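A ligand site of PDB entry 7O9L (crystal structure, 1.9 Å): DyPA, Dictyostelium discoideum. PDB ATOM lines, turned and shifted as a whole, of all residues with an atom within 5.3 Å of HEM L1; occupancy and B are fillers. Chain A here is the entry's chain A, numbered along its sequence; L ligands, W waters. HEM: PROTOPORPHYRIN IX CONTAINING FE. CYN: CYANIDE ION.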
ATOM      1  N   ASP A 148       2.915 -32.380  18.691  1.00  0.00           N
ATOM      2  CA  ASP A 148       2.079 -31.695  17.716  1.00  0.00           C
ATOM      3  C   ASP A 148       2.060 -32.518  16.426  1.00  0.00           C
ATOM      4  O   ASP A 148       2.911 -33.381  16.213  1.00  0.00           O
ATOM      5  CB  ASP A 148       2.625 -30.279  17.466  1.00  0.00           C
ATOM      6  CG  ASP A 148       1.903 -29.544  16.355  1.00  0.00           C
ATOM      7  OD1 ASP A 148       0.797 -29.018  16.599  1.00  0.00           O
ATOM      8  OD2 ASP A 148       2.448 -29.499  15.220  1.00  0.00           O
ATOM      9  N   THR A 150       3.007 -31.623  13.604  1.00  0.00           N
ATOM     10  CA  THR A 150       4.327 -31.538  12.968  1.00  0.00           C
ATOM     11  C   THR A 150       5.267 -32.648  13.433  1.00  0.00           C
ATOM     12  O   THR A 150       6.352 -32.797  12.850  1.00  0.00           O
ATOM     13  CB  THR A 150       4.998 -30.212  13.288  1.00  0.00           C
ATOM     14  OG1 THR A 150       5.075 -30.077  14.715  1.00  0.00           O
ATOM     15  CG2 THR A 150       4.213 -29.045  12.680  1.00  0.00           C
ATOM     16  N   PHE A 152       6.844 -32.672  16.269  1.00  0.00           N
ATOM     17  CA  PHE A 152       7.723 -32.146  17.313  1.00  0.00           C
ATOM     18  C   PHE A 152       6.988 -32.157  18.647  1.00  0.00           C
ATOM     19  O   PHE A 152       5.785 -31.908  18.711  1.00  0.00           O
ATOM     20  CB  PHE A 152       8.156 -30.702  16.968  1.00  0.00           C
ATOM     21  CG  PHE A 152       9.286 -30.639  15.994  1.00  0.00           C
ATOM     22  CD1 PHE A 152       9.097 -31.047  14.679  1.00  0.00           C
ATOM     23  CD2 PHE A 152      10.546 -30.193  16.386  1.00  0.00           C
ATOM     24  CE1 PHE A 152      10.163 -31.016  13.760  1.00  0.00           C
ATOM     25  CE2 PHE A 152      11.620 -30.153  15.472  1.00  0.00           C
ATOM     26  CZ  PHE A 152      11.418 -30.562  14.163  1.00  0.00           C
ATOM     27  N   ILE A 153       7.725 -32.451  19.719  1.00  0.00           N
ATOM     28  CA  ILE A 153       7.162 -32.376  21.063  1.00  0.00           C
ATOM     29  C   ILE A 153       6.727 -30.945  21.344  1.00  0.00           C
ATOM     30  O   ILE A 153       7.494 -30.002  21.146  1.00  0.00           O
ATOM     31  CB  ILE A 153       8.204 -32.827  22.097  1.00  0.00           C
ATOM     32  CG1 ILE A 153       8.558 -34.303  21.904  1.00  0.00           C
ATOM     33  CG2 ILE A 153       7.706 -32.558  23.522  1.00  0.00           C
ATOM     34  CD1 ILE A 153       9.819 -34.710  22.651  1.00  0.00           C
ATOM     35  N   ASP A 154       5.488 -30.769  21.828  1.00  0.00           N
ATOM     36  CA  ASP A 154       4.965 -29.457  22.195  1.00  0.00           C
ATOM     37  C   ASP A 154       4.880 -29.360  23.719  1.00  0.00           C
ATOM     38  O   ASP A 154       4.170 -30.160  24.345  1.00  0.00           O
ATOM     39  CB  ASP A 154       3.599 -29.214  21.553  1.00  0.00           C
ATOM     40  CG  ASP A 154       3.096 -27.798  21.743  1.00  0.00           C
ATOM     41  OD1 ASP A 154       3.932 -26.876  21.898  1.00  0.00           O
ATOM     42  OD2 ASP A 154       1.852 -27.597  21.736  1.00  0.00           O
ATOM     43  N   GLY A 155       5.603 -28.401  24.308  1.00  0.00           N
ATOM     44  CA  GLY A 155       5.511 -28.174  25.747  1.00  0.00           C
ATOM     45  C   GLY A 155       6.829 -28.145  26.496  1.00  0.00           C
ATOM     46  O   GLY A 155       6.844 -27.849  27.698  1.00  0.00           O
ATOM     47  N   THR A 156       7.941 -28.395  25.805  1.00  0.00           N
ATOM     48  CA  THR A 156       9.247 -28.512  26.485  1.00  0.00           C
ATOM     49  C   THR A 156       9.551 -27.319  27.393  1.00  0.00           C
ATOM     50  O   THR A 156       9.980 -27.499  28.537  1.00  0.00           O
ATOM     51  CB  THR A 156      10.353 -28.677  25.444  1.00  0.00           C
ATOM     52  OG1 THR A 156      10.029 -29.779  24.588  1.00  0.00           O
ATOM     53  CG2 THR A 156      11.680 -28.965  26.125  1.00  0.00           C
ATOM     54  N   GLU A 157       9.352 -26.090  26.901  1.00  0.00           N
ATOM     55  CA  GLU A 157       9.656 -24.900  27.699  1.00  0.00           C
ATOM     56  C   GLU A 157       8.413 -24.251  28.309  1.00  0.00           C
ATOM     57  O   GLU A 157       8.481 -23.109  28.760  1.00  0.00           O
ATOM     58  CB  GLU A 157      10.409 -23.868  26.843  1.00  0.00           C
ATOM     59  CG  GLU A 157      11.796 -24.347  26.421  1.00  0.00           C
ATOM     60  CD  GLU A 157      12.754 -24.514  27.594  1.00  0.00           C
ATOM     61  OE1 GLU A 157      12.625 -23.771  28.588  1.00  0.00           O
ATOM     62  OE2 GLU A 157      13.629 -25.400  27.521  1.00  0.00           O
ATOM     63  N   ASN A 158       7.291 -24.958  28.325  1.00  0.00           N
ATOM     64  CA  ASN A 158       6.125 -24.492  29.060  1.00  0.00           C
ATOM     65  C   ASN A 158       6.472 -24.420  30.539  1.00  0.00           C
ATOM     66  O   ASN A 158       7.059 -25.375  31.073  1.00  0.00           O
ATOM     67  CB  ASN A 158       4.976 -25.481  28.825  1.00  0.00           C
ATOM     68  CG  ASN A 158       3.612 -24.829  28.776  1.00  0.00           C
ATOM     69  OD1 ASN A 158       3.453 -23.609  28.701  1.00  0.00           O
ATOM     70  ND2 ASN A 158       2.584 -25.679  28.790  1.00  0.00           N
ATOM     71  N   PHE A 184      -5.842 -16.450  25.265  1.00  0.00           N
ATOM     72  CA  PHE A 184      -5.869 -16.315  23.817  1.00  0.00           C
ATOM     73  C   PHE A 184      -6.091 -17.697  23.211  1.00  0.00           C
ATOM     74  O   PHE A 184      -5.363 -18.647  23.533  1.00  0.00           O
ATOM     75  CB  PHE A 184      -4.545 -15.712  23.304  1.00  0.00           C
ATOM     76  CG  PHE A 184      -4.384 -15.733  21.798  1.00  0.00           C
ATOM     77  CD1 PHE A 184      -5.236 -14.995  20.981  1.00  0.00           C
ATOM     78  CD2 PHE A 184      -3.352 -16.463  21.214  1.00  0.00           C
ATOM     79  CE1 PHE A 184      -5.083 -14.995  19.605  1.00  0.00           C
ATOM     80  CE2 PHE A 184      -3.178 -16.467  19.831  1.00  0.00           C
ATOM     81  CZ  PHE A 184      -4.034 -15.721  19.026  1.00  0.00           C
ATOM     82  N   GLN A 186      -6.652 -19.789  19.392  1.00  0.00           N
ATOM     83  CA  GLN A 186      -6.377 -19.620  17.970  1.00  0.00           C
ATOM     84  C   GLN A 186      -6.305 -20.999  17.345  1.00  0.00           C
ATOM     85  O   GLN A 186      -5.420 -21.782  17.684  1.00  0.00           O
ATOM     86  CB  GLN A 186      -5.046 -18.879  17.784  1.00  0.00           C
ATOM     87  CG  GLN A 186      -4.699 -18.515  16.351  1.00  0.00           C
ATOM     88  CD  GLN A 186      -3.494 -17.583  16.268  1.00  0.00           C
ATOM     89  OE1 GLN A 186      -2.452 -17.843  16.890  1.00  0.00           O
ATOM     90  NE2 GLN A 186      -3.627 -16.481  15.517  1.00  0.00           N
ATOM     91  N   TYR A 188      -5.369 -23.483  14.430  1.00  0.00           N
ATOM     92  CA  TYR A 188      -4.480 -23.600  13.276  1.00  0.00           C
ATOM     93  C   TYR A 188      -4.879 -24.796  12.418  1.00  0.00           C
ATOM     94  O   TYR A 188      -5.213 -25.862  12.938  1.00  0.00           O
ATOM     95  CB  TYR A 188      -3.023 -23.768  13.698  1.00  0.00           C
ATOM     96  CG  TYR A 188      -2.391 -22.469  14.117  1.00  0.00           C
ATOM     97  CD1 TYR A 188      -2.577 -21.957  15.401  1.00  0.00           C
ATOM     98  CD2 TYR A 188      -1.605 -21.729  13.222  1.00  0.00           C
ATOM     99  CE1 TYR A 188      -2.001 -20.755  15.789  1.00  0.00           C
ATOM    100  CE2 TYR A 188      -1.020 -20.543  13.588  1.00  0.00           C
ATOM    101  CZ  TYR A 188      -1.228 -20.059  14.866  1.00  0.00           C
ATOM    102  OH  TYR A 188      -0.642 -18.868  15.219  1.00  0.00           O
ATOM    103  N   HIS A 190      -3.085 -27.205   9.772  1.00  0.00           N
ATOM    104  CA  HIS A 190      -1.770 -27.604   9.259  1.00  0.00           C
ATOM    105  C   HIS A 190      -1.865 -28.053   7.807  1.00  0.00           C
ATOM    106  O   HIS A 190      -2.849 -28.663   7.378  1.00  0.00           O
ATOM    107  CB  HIS A 190      -1.194 -28.763  10.069  1.00  0.00           C
ATOM    108  CG  HIS A 190      -0.742 -28.395  11.444  1.00  0.00           C
ATOM    109  ND1 HIS A 190      -0.987 -27.162  12.019  1.00  0.00           N
ATOM    110  CD2 HIS A 190      -0.035 -29.100  12.365  1.00  0.00           C
ATOM    111  CE1 HIS A 190      -0.458 -27.129  13.225  1.00  0.00           C
ATOM    112  NE2 HIS A 190       0.126 -28.290  13.459  1.00  0.00           N
ATOM    113  N   VAL A 207      11.489 -25.002  13.612  1.00  0.00           N
ATOM    114  CA  VAL A 207      11.014 -24.970  14.987  1.00  0.00           C
ATOM    115  C   VAL A 207      12.053 -24.333  15.895  1.00  0.00           C
ATOM    116  O   VAL A 207      11.724 -23.498  16.757  1.00  0.00           O
ATOM    117  CB  VAL A 207      10.667 -26.399  15.448  1.00  0.00           C
ATOM    118  CG1 VAL A 207      10.305 -26.435  16.938  1.00  0.00           C
ATOM    119  CG2 VAL A 207       9.547 -26.986  14.582  1.00  0.00           C
ATOM    120  N   ARG A 209      14.307 -26.466  17.627  1.00  0.00           N
ATOM    121  CA  ARG A 209      14.706 -27.543  18.520  1.00  0.00           C
ATOM    122  C   ARG A 209      14.879 -28.805  17.694  1.00  0.00           C
ATOM    123  O   ARG A 209      14.401 -28.888  16.557  1.00  0.00           O
ATOM    124  CB  ARG A 209      13.680 -27.778  19.651  1.00  0.00           C
ATOM    125  CG  ARG A 209      13.160 -26.494  20.323  1.00  0.00           C
ATOM    126  CD  ARG A 209      12.276 -26.848  21.537  1.00  0.00           C
ATOM    127  NE  ARG A 209      13.106 -27.386  22.611  1.00  0.00           N
ATOM    128  CZ  ARG A 209      13.709 -26.640  23.544  1.00  0.00           C
ATOM    129  NH1 ARG A 209      13.565 -25.323  23.550  1.00  0.00           N
ATOM    130  NH2 ARG A 209      14.460 -27.220  24.461  1.00  0.00           N
ATOM    131  N   SER A 214      13.788 -32.847  21.335  1.00  0.00           N
ATOM    132  CA  SER A 214      13.428 -31.461  21.652  1.00  0.00           C
ATOM    133  C   SER A 214      14.565 -30.753  22.393  1.00  0.00           C
ATOM    134  O   SER A 214      14.348 -30.037  23.373  1.00  0.00           O
ATOM    135  CB  SER A 214      12.123 -31.385  22.441  1.00  0.00           C
ATOM    136  OG  SER A 214      11.639 -30.046  22.455  1.00  0.00           O
ATOM    137  N   HIS A 227      10.745 -20.729  15.143  1.00  0.00           N
ATOM    138  CA  HIS A 227       9.617 -20.504  16.045  1.00  0.00           C
ATOM    139  C   HIS A 227      10.099 -20.156  17.446  1.00  0.00           C
ATOM    140  O   HIS A 227       9.584 -19.215  18.069  1.00  0.00           O
ATOM    141  CB  HIS A 227       8.728 -21.737  16.054  1.00  0.00           C
ATOM    142  CG  HIS A 227       7.510 -21.562  16.894  1.00  0.00           C
ATOM    143  ND1 HIS A 227       6.613 -20.532  16.686  1.00  0.00           N
ATOM    144  CD2 HIS A 227       7.056 -22.261  17.945  1.00  0.00           C
ATOM    145  CE1 HIS A 227       5.646 -20.627  17.582  1.00  0.00           C
ATOM    146  NE2 HIS A 227       5.898 -21.666  18.358  1.00  0.00           N
ATOM    147  N   VAL A 228      11.119 -20.857  17.943  1.00  0.00           N
ATOM    148  CA  VAL A 228      11.654 -20.553  19.278  1.00  0.00           C
ATOM    149  C   VAL A 228      12.264 -19.149  19.315  1.00  0.00           C
ATOM    150  O   VAL A 228      12.098 -18.415  20.293  1.00  0.00           O
ATOM    151  CB  VAL A 228      12.652 -21.633  19.724  1.00  0.00           C
ATOM    152  CG1 VAL A 228      13.370 -21.194  20.997  1.00  0.00           C
ATOM    153  CG2 VAL A 228      11.923 -22.960  19.936  1.00  0.00           C
ATOM    154  N   THR A 231       9.387 -16.641  19.683  1.00  0.00           N
ATOM    155  CA  THR A 231       8.521 -16.662  20.851  1.00  0.00           C
ATOM    156  C   THR A 231       9.253 -16.599  22.179  1.00  0.00           C
ATOM    157  O   THR A 231       8.608 -16.346  23.202  1.00  0.00           O
ATOM    158  CB  THR A 231       7.630 -17.911  20.854  1.00  0.00           C
ATOM    159  OG1 THR A 231       8.458 -19.088  20.839  1.00  0.00           O
ATOM    160  CG2 THR A 231       6.670 -17.923  19.660  1.00  0.00           C
ATOM    161  N   ASP A 232      10.556 -16.858  22.199  1.00  0.00           N
ATOM    162  CA  ASP A 232      11.329 -16.786  23.442  1.00  0.00           C
ATOM    163  C   ASP A 232      11.801 -15.344  23.602  1.00  0.00           C
ATOM    164  O   ASP A 232      12.884 -14.972  23.166  1.00  0.00           O
ATOM    165  CB  ASP A 232      12.494 -17.765  23.387  1.00  0.00           C
ATOM    166  CG  ASP A 232      13.364 -17.718  24.631  1.00  0.00           C
ATOM    167  OD1 ASP A 232      12.933 -17.139  25.653  1.00  0.00           O
ATOM    168  OD2 ASP A 232      14.489 -18.272  24.585  1.00  0.00           O
ATOM    169  N   LYS A 241       6.987 -15.048  29.503  1.00  0.00           N
ATOM    170  CA  LYS A 241       6.503 -16.413  29.428  1.00  0.00           C
ATOM    171  C   LYS A 241       4.974 -16.462  29.530  1.00  0.00           C
ATOM    172  O   LYS A 241       4.322 -15.562  30.074  1.00  0.00           O
ATOM    173  CB  LYS A 241       7.134 -17.263  30.526  1.00  0.00           C
ATOM    174  CG  LYS A 241       8.649 -17.432  30.362  1.00  0.00           C
ATOM    175  CD  LYS A 241       9.203 -18.448  31.344  1.00  0.00           C
ATOM    176  CE  LYS A 241      10.707 -18.587  31.199  1.00  0.00           C
ATOM    177  NZ  LYS A 241      11.095 -19.065  29.838  1.00  0.00           N
ATOM    178  N   ILE A 242       4.402 -17.555  29.003  1.00  0.00           N
ATOM    179  CA  ILE A 242       2.961 -17.794  29.007  1.00  0.00           C
ATOM    180  C   ILE A 242       2.754 -19.255  29.332  1.00  0.00           C
ATOM    181  O   ILE A 242       3.684 -20.060  29.283  1.00  0.00           O
ATOM    182  CB  ILE A 242       2.306 -17.437  27.655  1.00  0.00           C
ATOM    183  CG1 ILE A 242       2.896 -18.320  26.556  1.00  0.00           C
ATOM    184  CG2 ILE A 242       2.527 -15.934  27.303  1.00  0.00           C
ATOM    185  CD1 ILE A 242       2.321 -18.064  25.164  1.00  0.00           C
ATOM    186  N   ARG A 244       0.836 -22.439  28.083  1.00  0.00           N
ATOM    187  CA  ARG A 244       0.097 -22.995  26.958  1.00  0.00           C
ATOM    188  C   ARG A 244      -0.631 -24.274  27.368  1.00  0.00           C
ATOM    189  O   ARG A 244      -0.077 -25.097  28.115  1.00  0.00           O
ATOM    190  CB  ARG A 244       1.026 -23.285  25.776  1.00  0.00           C
ATOM    191  CG  ARG A 244       1.586 -21.967  25.147  1.00  0.00           C
ATOM    192  CD  ARG A 244       2.749 -22.297  24.191  1.00  0.00           C
ATOM    193  NE  ARG A 244       3.980 -22.654  24.916  1.00  0.00           N
ATOM    194  CZ  ARG A 244       4.779 -23.675  24.609  1.00  0.00           C
ATOM    195  NH1 ARG A 244       4.499 -24.475  23.583  1.00  0.00           N
ATOM    196  NH2 ARG A 244       5.860 -23.899  25.350  1.00  0.00           N
ATOM    197  N   LEU A 258      -3.607 -27.645  15.195  1.00  0.00           N
ATOM    198  CA  LEU A 258      -3.370 -27.385  16.616  1.00  0.00           C
ATOM    199  C   LEU A 258      -4.417 -26.404  17.109  1.00  0.00           C
ATOM    200  O   LEU A 258      -4.604 -25.334  16.530  1.00  0.00           O
ATOM    201  CB  LEU A 258      -1.954 -26.812  16.848  1.00  0.00           C
ATOM    202  CG  LEU A 258      -1.652 -26.551  18.331  1.00  0.00           C
ATOM    203  CD1 LEU A 258      -1.416 -27.882  19.076  1.00  0.00           C
ATOM    204  CD2 LEU A 258      -0.450 -25.611  18.513  1.00  0.00           C
ATOM    205  N   PHE A 260      -4.606 -23.936  19.542  1.00  0.00           N
ATOM    206  CA  PHE A 260      -3.709 -23.213  20.430  1.00  0.00           C
ATOM    207  C   PHE A 260      -4.501 -22.489  21.516  1.00  0.00           C
ATOM    208  O   PHE A 260      -5.509 -21.830  21.234  1.00  0.00           O
ATOM    209  CB  PHE A 260      -2.896 -22.172  19.648  1.00  0.00           C
ATOM    210  CG  PHE A 260      -1.922 -21.440  20.503  1.00  0.00           C
ATOM    211  CD1 PHE A 260      -0.649 -21.956  20.721  1.00  0.00           C
ATOM    212  CD2 PHE A 260      -2.270 -20.254  21.131  1.00  0.00           C
ATOM    213  CE1 PHE A 260       0.251 -21.306  21.526  1.00  0.00           C
ATOM    214  CE2 PHE A 260      -1.360 -19.588  21.928  1.00  0.00           C
ATOM    215  CZ  PHE A 260      -0.108 -20.127  22.127  1.00  0.00           C
ATOM    216  N   ILE A 270       1.406 -12.291  25.627  1.00  0.00           N
ATOM    217  CA  ILE A 270       0.900 -12.993  24.445  1.00  0.00           C
ATOM    218  C   ILE A 270       1.006 -12.116  23.212  1.00  0.00           C
ATOM    219  O   ILE A 270       1.534 -12.533  22.177  1.00  0.00           O
ATOM    220  CB  ILE A 270      -0.560 -13.431  24.672  1.00  0.00           C
ATOM    221  CG1 ILE A 270      -0.645 -14.374  25.880  1.00  0.00           C
ATOM    222  CG2 ILE A 270      -1.105 -14.098  23.409  1.00  0.00           C
ATOM    223  CD1 ILE A 270      -2.080 -14.685  26.309  1.00  0.00           C
ATOM    224  N   GLN A 273       4.317 -11.712  21.516  1.00  0.00           N
ATOM    225  CA  GLN A 273       4.716 -12.877  20.740  1.00  0.00           C
ATOM    226  C   GLN A 273       3.981 -12.927  19.411  1.00  0.00           C
ATOM    227  O   GLN A 273       4.557 -13.337  18.399  1.00  0.00           O
ATOM    228  CB  GLN A 273       4.467 -14.154  21.544  1.00  0.00           C
ATOM    229  CG  GLN A 273       5.374 -14.266  22.758  1.00  0.00           C
ATOM    230  CD  GLN A 273       5.169 -15.569  23.495  1.00  0.00           C
ATOM    231  OE1 GLN A 273       4.915 -16.593  22.879  1.00  0.00           O
ATOM    232  NE2 GLN A 273       5.262 -15.536  24.820  1.00  0.00           N
ATOM    233  N   LEU A 274       2.701 -12.538  19.393  1.00  0.00           N
ATOM    234  CA  LEU A 274       1.971 -12.482  18.123  1.00  0.00           C
ATOM    235  C   LEU A 274       2.563 -11.437  17.185  1.00  0.00           C
ATOM    236  O   LEU A 274       2.669 -11.674  15.975  1.00  0.00           O
ATOM    237  CB  LEU A 274       0.486 -12.182  18.375  1.00  0.00           C
ATOM    238  CG  LEU A 274      -0.262 -13.260  19.174  1.00  0.00           C
ATOM    239  CD1 LEU A 274      -1.712 -12.835  19.436  1.00  0.00           C
ATOM    240  CD2 LEU A 274      -0.193 -14.602  18.464  1.00  0.00           C
ATOM    241  N   MET A 277       5.661 -13.158  15.737  1.00  0.00           N
ATOM    242  CA  MET A 277       5.414 -14.252  14.793  1.00  0.00           C
ATOM    243  C   MET A 277       4.869 -13.728  13.477  1.00  0.00           C
ATOM    244  O   MET A 277       5.180 -14.267  12.404  1.00  0.00           O
ATOM    245  CB  MET A 277       4.433 -15.263  15.392  1.00  0.00           C
ATOM    246  CG  MET A 277       5.032 -16.115  16.471  1.00  0.00           C
ATOM    247  SD  MET A 277       3.768 -17.154  17.233  1.00  0.00           S
ATOM    248  CE  MET A 277       3.266 -18.152  15.815  1.00  0.00           C
ATOM    249  N   LEU A 288       7.231 -21.253  10.939  1.00  0.00           N
ATOM    250  CA  LEU A 288       6.158 -22.239  11.061  1.00  0.00           C
ATOM    251  C   LEU A 288       4.959 -21.859  10.217  1.00  0.00           C
ATOM    252  O   LEU A 288       4.200 -22.720   9.773  1.00  0.00           O
ATOM    253  CB  LEU A 288       5.737 -22.393  12.526  1.00  0.00           C
ATOM    254  CG  LEU A 288       6.146 -23.620  13.343  1.00  0.00           C
ATOM    255  CD1 LEU A 288       5.337 -23.633  14.630  1.00  0.00           C
ATOM    256  CD2 LEU A 288       5.972 -24.932  12.579  1.00  0.00           C
ATOM    257  N   THR A 292       1.378 -23.807   8.318  1.00  0.00           N
ATOM    258  CA  THR A 292       0.141 -23.834   9.072  1.00  0.00           C
ATOM    259  C   THR A 292      -0.469 -22.442   9.024  1.00  0.00           C
ATOM    260  O   THR A 292       0.235 -21.453   8.784  1.00  0.00           O
ATOM    261  CB  THR A 292       0.386 -24.283  10.523  1.00  0.00           C
ATOM    262  OG1 THR A 292      -0.874 -24.497  11.189  1.00  0.00           O
ATOM    263  CG2 THR A 292       1.203 -23.233  11.284  1.00  0.00           C
HETATM  264  CHA HEM L   1       7.353 -23.488  21.713  1.00  0.00           C
HETATM  265  CHB HEM L   1       4.691 -25.640  18.249  1.00  0.00           C
HETATM  266  CHC HEM L   1       1.929 -21.607  17.915  1.00  0.00           C
HETATM  267  CHD HEM L   1       4.217 -19.762  21.770  1.00  0.00           C
HETATM  268  C1A HEM L   1       6.861 -24.373  20.781  1.00  0.00           C
HETATM  269  C2A HEM L   1       7.499 -25.596  20.456  1.00  0.00           C
HETATM  270  C3A HEM L   1       6.748 -26.194  19.490  1.00  0.00           C
HETATM  271  C4A HEM L   1       5.636 -25.355  19.216  1.00  0.00           C
HETATM  272  CMA HEM L   1       7.040 -27.527  18.832  1.00  0.00           C
HETATM  273  CAA HEM L   1       8.794 -26.122  21.065  1.00  0.00           C
HETATM  274  CBA HEM L   1       8.583 -26.993  22.327  1.00  0.00           C
HETATM  275  CGA HEM L   1       8.151 -26.160  23.508  1.00  0.00           C
HETATM  276  O1A HEM L   1       8.988 -25.508  24.183  1.00  0.00           O
HETATM  277  O2A HEM L   1       6.948 -26.128  23.836  1.00  0.00           O
HETATM  278  C1B HEM L   1       3.726 -24.698  17.858  1.00  0.00           C
HETATM  279  C2B HEM L   1       2.788 -24.932  16.798  1.00  0.00           C
HETATM  280  C3B HEM L   1       2.011 -23.793  16.703  1.00  0.00           C
HETATM  281  C4B HEM L   1       2.511 -22.876  17.734  1.00  0.00           C
HETATM  282  CMB HEM L   1       2.708 -26.206  15.976  1.00  0.00           C
HETATM  283  CAB HEM L   1       0.894 -23.457  15.805  1.00  0.00           C
HETATM  284  CBB HEM L   1       0.746 -24.006  14.598  1.00  0.00           C
HETATM  285  C1C HEM L   1       2.285 -20.742  18.939  1.00  0.00           C
HETATM  286  C2C HEM L   1       1.748 -19.467  19.189  1.00  0.00           C
HETATM  287  C3C HEM L   1       2.408 -18.944  20.299  1.00  0.00           C
HETATM  288  C4C HEM L   1       3.365 -19.915  20.700  1.00  0.00           C
HETATM  289  CMC HEM L   1       0.627 -18.831  18.384  1.00  0.00           C
HETATM  290  CAC HEM L   1       2.238 -17.605  20.972  1.00  0.00           C
HETATM  291  CBC HEM L   1       1.116 -16.893  20.999  1.00  0.00           C
HETATM  292  C1D HEM L   1       5.242 -20.692  22.035  1.00  0.00           C
HETATM  293  C2D HEM L   1       6.179 -20.437  23.134  1.00  0.00           C
HETATM  294  C3D HEM L   1       7.062 -21.458  23.113  1.00  0.00           C
HETATM  295  C4D HEM L   1       6.658 -22.332  22.011  1.00  0.00           C
HETATM  296  CMD HEM L   1       6.170 -19.261  24.082  1.00  0.00           C
HETATM  297  CAD HEM L   1       8.233 -21.652  24.054  1.00  0.00           C
HETATM  298  CBD HEM L   1       9.418 -20.829  23.531  1.00  0.00           C
HETATM  299  CGD HEM L   1      10.566 -20.882  24.512  1.00  0.00           C
HETATM  300  O1D HEM L   1      10.573 -20.127  25.503  1.00  0.00           O
HETATM  301  O2D HEM L   1      11.511 -21.678  24.322  1.00  0.00           O
HETATM  302  NA  HEM L   1       5.752 -24.212  19.957  1.00  0.00           N
HETATM  303  NB  HEM L   1       3.513 -23.494  18.394  1.00  0.00           N
HETATM  304  NC  HEM L   1       3.289 -20.971  19.822  1.00  0.00           N
HETATM  305  ND  HEM L   1       5.535 -21.867  21.404  1.00  0.00           N
HETATM  306 FE   HEM L   1       4.615 -22.569  19.891  1.00  0.00          FE
HETATM  307  C   CYN L   2       2.511 -24.093  21.263  1.00  0.00           C
HETATM  308  N   CYN L   2       1.395 -24.598  21.856  1.00  0.00           N
HETATM  309  O   HOH W   1      12.397 -20.245  27.590  1.00  0.00           O
HETATM  310  O   HOH W   2      14.006 -21.385  25.310  1.00  0.00           O
HETATM  311  O   HOH W   3       8.896 -18.252  26.302  1.00  0.00           O
HETATM  312  O   HOH W   4       8.941 -20.532  28.387  1.00  0.00           O
HETATM  313  O   HOH W   5      11.121 -24.063  23.127  1.00  0.00           O
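NE2 of His 227 is bound to FE of HEM L1 (2.2 Å).
O2A of HEM L1 is in hydrogen-bond range of N of Gly 155 (2.7 Å).
An oxygen (O1A) of HEM L1 is in hydrogen-bond range of the backbone NH (N) of Glu 157 (2.8 Å).
O2A of HEM L1 is in salt-bridge range of NH2 of Arg 244 (2.9 Å).
N of Thr 156 is in hydrogen-bond range of O2A of HEM L1 (3.2 Å).
O of His 227 sits at hydrogen-bond distance from OG1 of Thr 231 (3.0 Å).
The backbone NH (N) of His 227 is in hydrogen-bond range of the backbone carbonyl oxygen (O) of Val 207 (3.4 Å).
The side-chain hydroxyl of Ser 214 is in hydrogen-bond range of the side-chain hydroxyl of Thr 156, at 2.7 Å.
OD2 of Asp 148 is in hydrogen-bond range of NE2 of His 190 (3.2 Å).
The side-chain carboxylate (OD2) of Asp 148 sits at hydrogen-bond distance from the backbone NH (N) of Thr 150.
N of Tyr 188 lies within hydrogen-bond range of O of Leu 258, at 2.9 Å.
The side-chain hydroxyl (OH) of Tyr 188 is in hydrogen-bond range of the side-chain amide oxygen (OE1) of Gln 186, 2.7 Å away.
N of Val 228 sits at hydrogen-bond distance from O of Val 207, at 3.0 Å.
Asp 148 touches HEM L1 (OD2 to CMB, 3.4 Å).
CB of Phe 152 touches CMA of HEM L1, 3.8 Å away.
Ile 153 touches HEM L1.
Asp 154 touches HEM L1.
Gln 186 touches HEM L1.
Tyr 188 touches HEM L1 (OH to CMC, 3.4 Å).
CE1 of His 190 touches CBB of HEM L1, 3.6 Å away.
Val 207 touches HEM L1 (CG1 to CMA, 3.9 Å).
Arg 209 touches HEM L1 (CD to CAA, 3.6 Å).
CG1 of Val 228 touches O2D of HEM L1, at 3.8 Å.
OG1 of Thr 231 touches CBD of HEM L1 (3.3 Å).
Asp 232 touches HEM L1.
Leu 258 touches HEM L1 (CD2 to C3B, 3.6 Å).
Phe 260 touches HEM L1 (CZ to C3C, 3.3 Å).
OE1 of Gln 273 touches CMD of HEM L1 (3.2 Å).
Leu 274 touches HEM L1.
SD of Met 277 touches C2C of HEM L1, at 3.6 Å.
Leu 288 touches HEM L1 (CD1 to C2B, 3.6 Å).
CG2 of Thr 292 touches CBB of HEM L1, 3.4 Å away.
Hydrophobic or aromatic side chains that line HEM L1: Phe 152, Tyr 188, His 190, Val 207, His 227, Val 228, Leu 258, Phe 260, Leu 274, Met 277 and Leu 288.
Water W5 bridges an oxygen (O2D) of HEM L1 (2.7 Å) and the guanidinium group (NH1) of Arg 209 (2.8 Å).
Water W2 lies within hydrogen-bond range of O2D of HEM L1 (2.7 Å) and OD2 of Asp 232 (3.2 Å).
Water W1 bridges O1D of HEM L1 (2.8 Å) and NZ of Lys 241 (2.9 Å).
Water W4 lies within hydrogen-bond range of the backbone carbonyl oxygen (O) of Glu 157 (2.6 Å), the side-chain amino group (NZ) of Lys 241 (3.0 Å) and an oxygen (O1D) of HEM L1 (3.3 Å).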
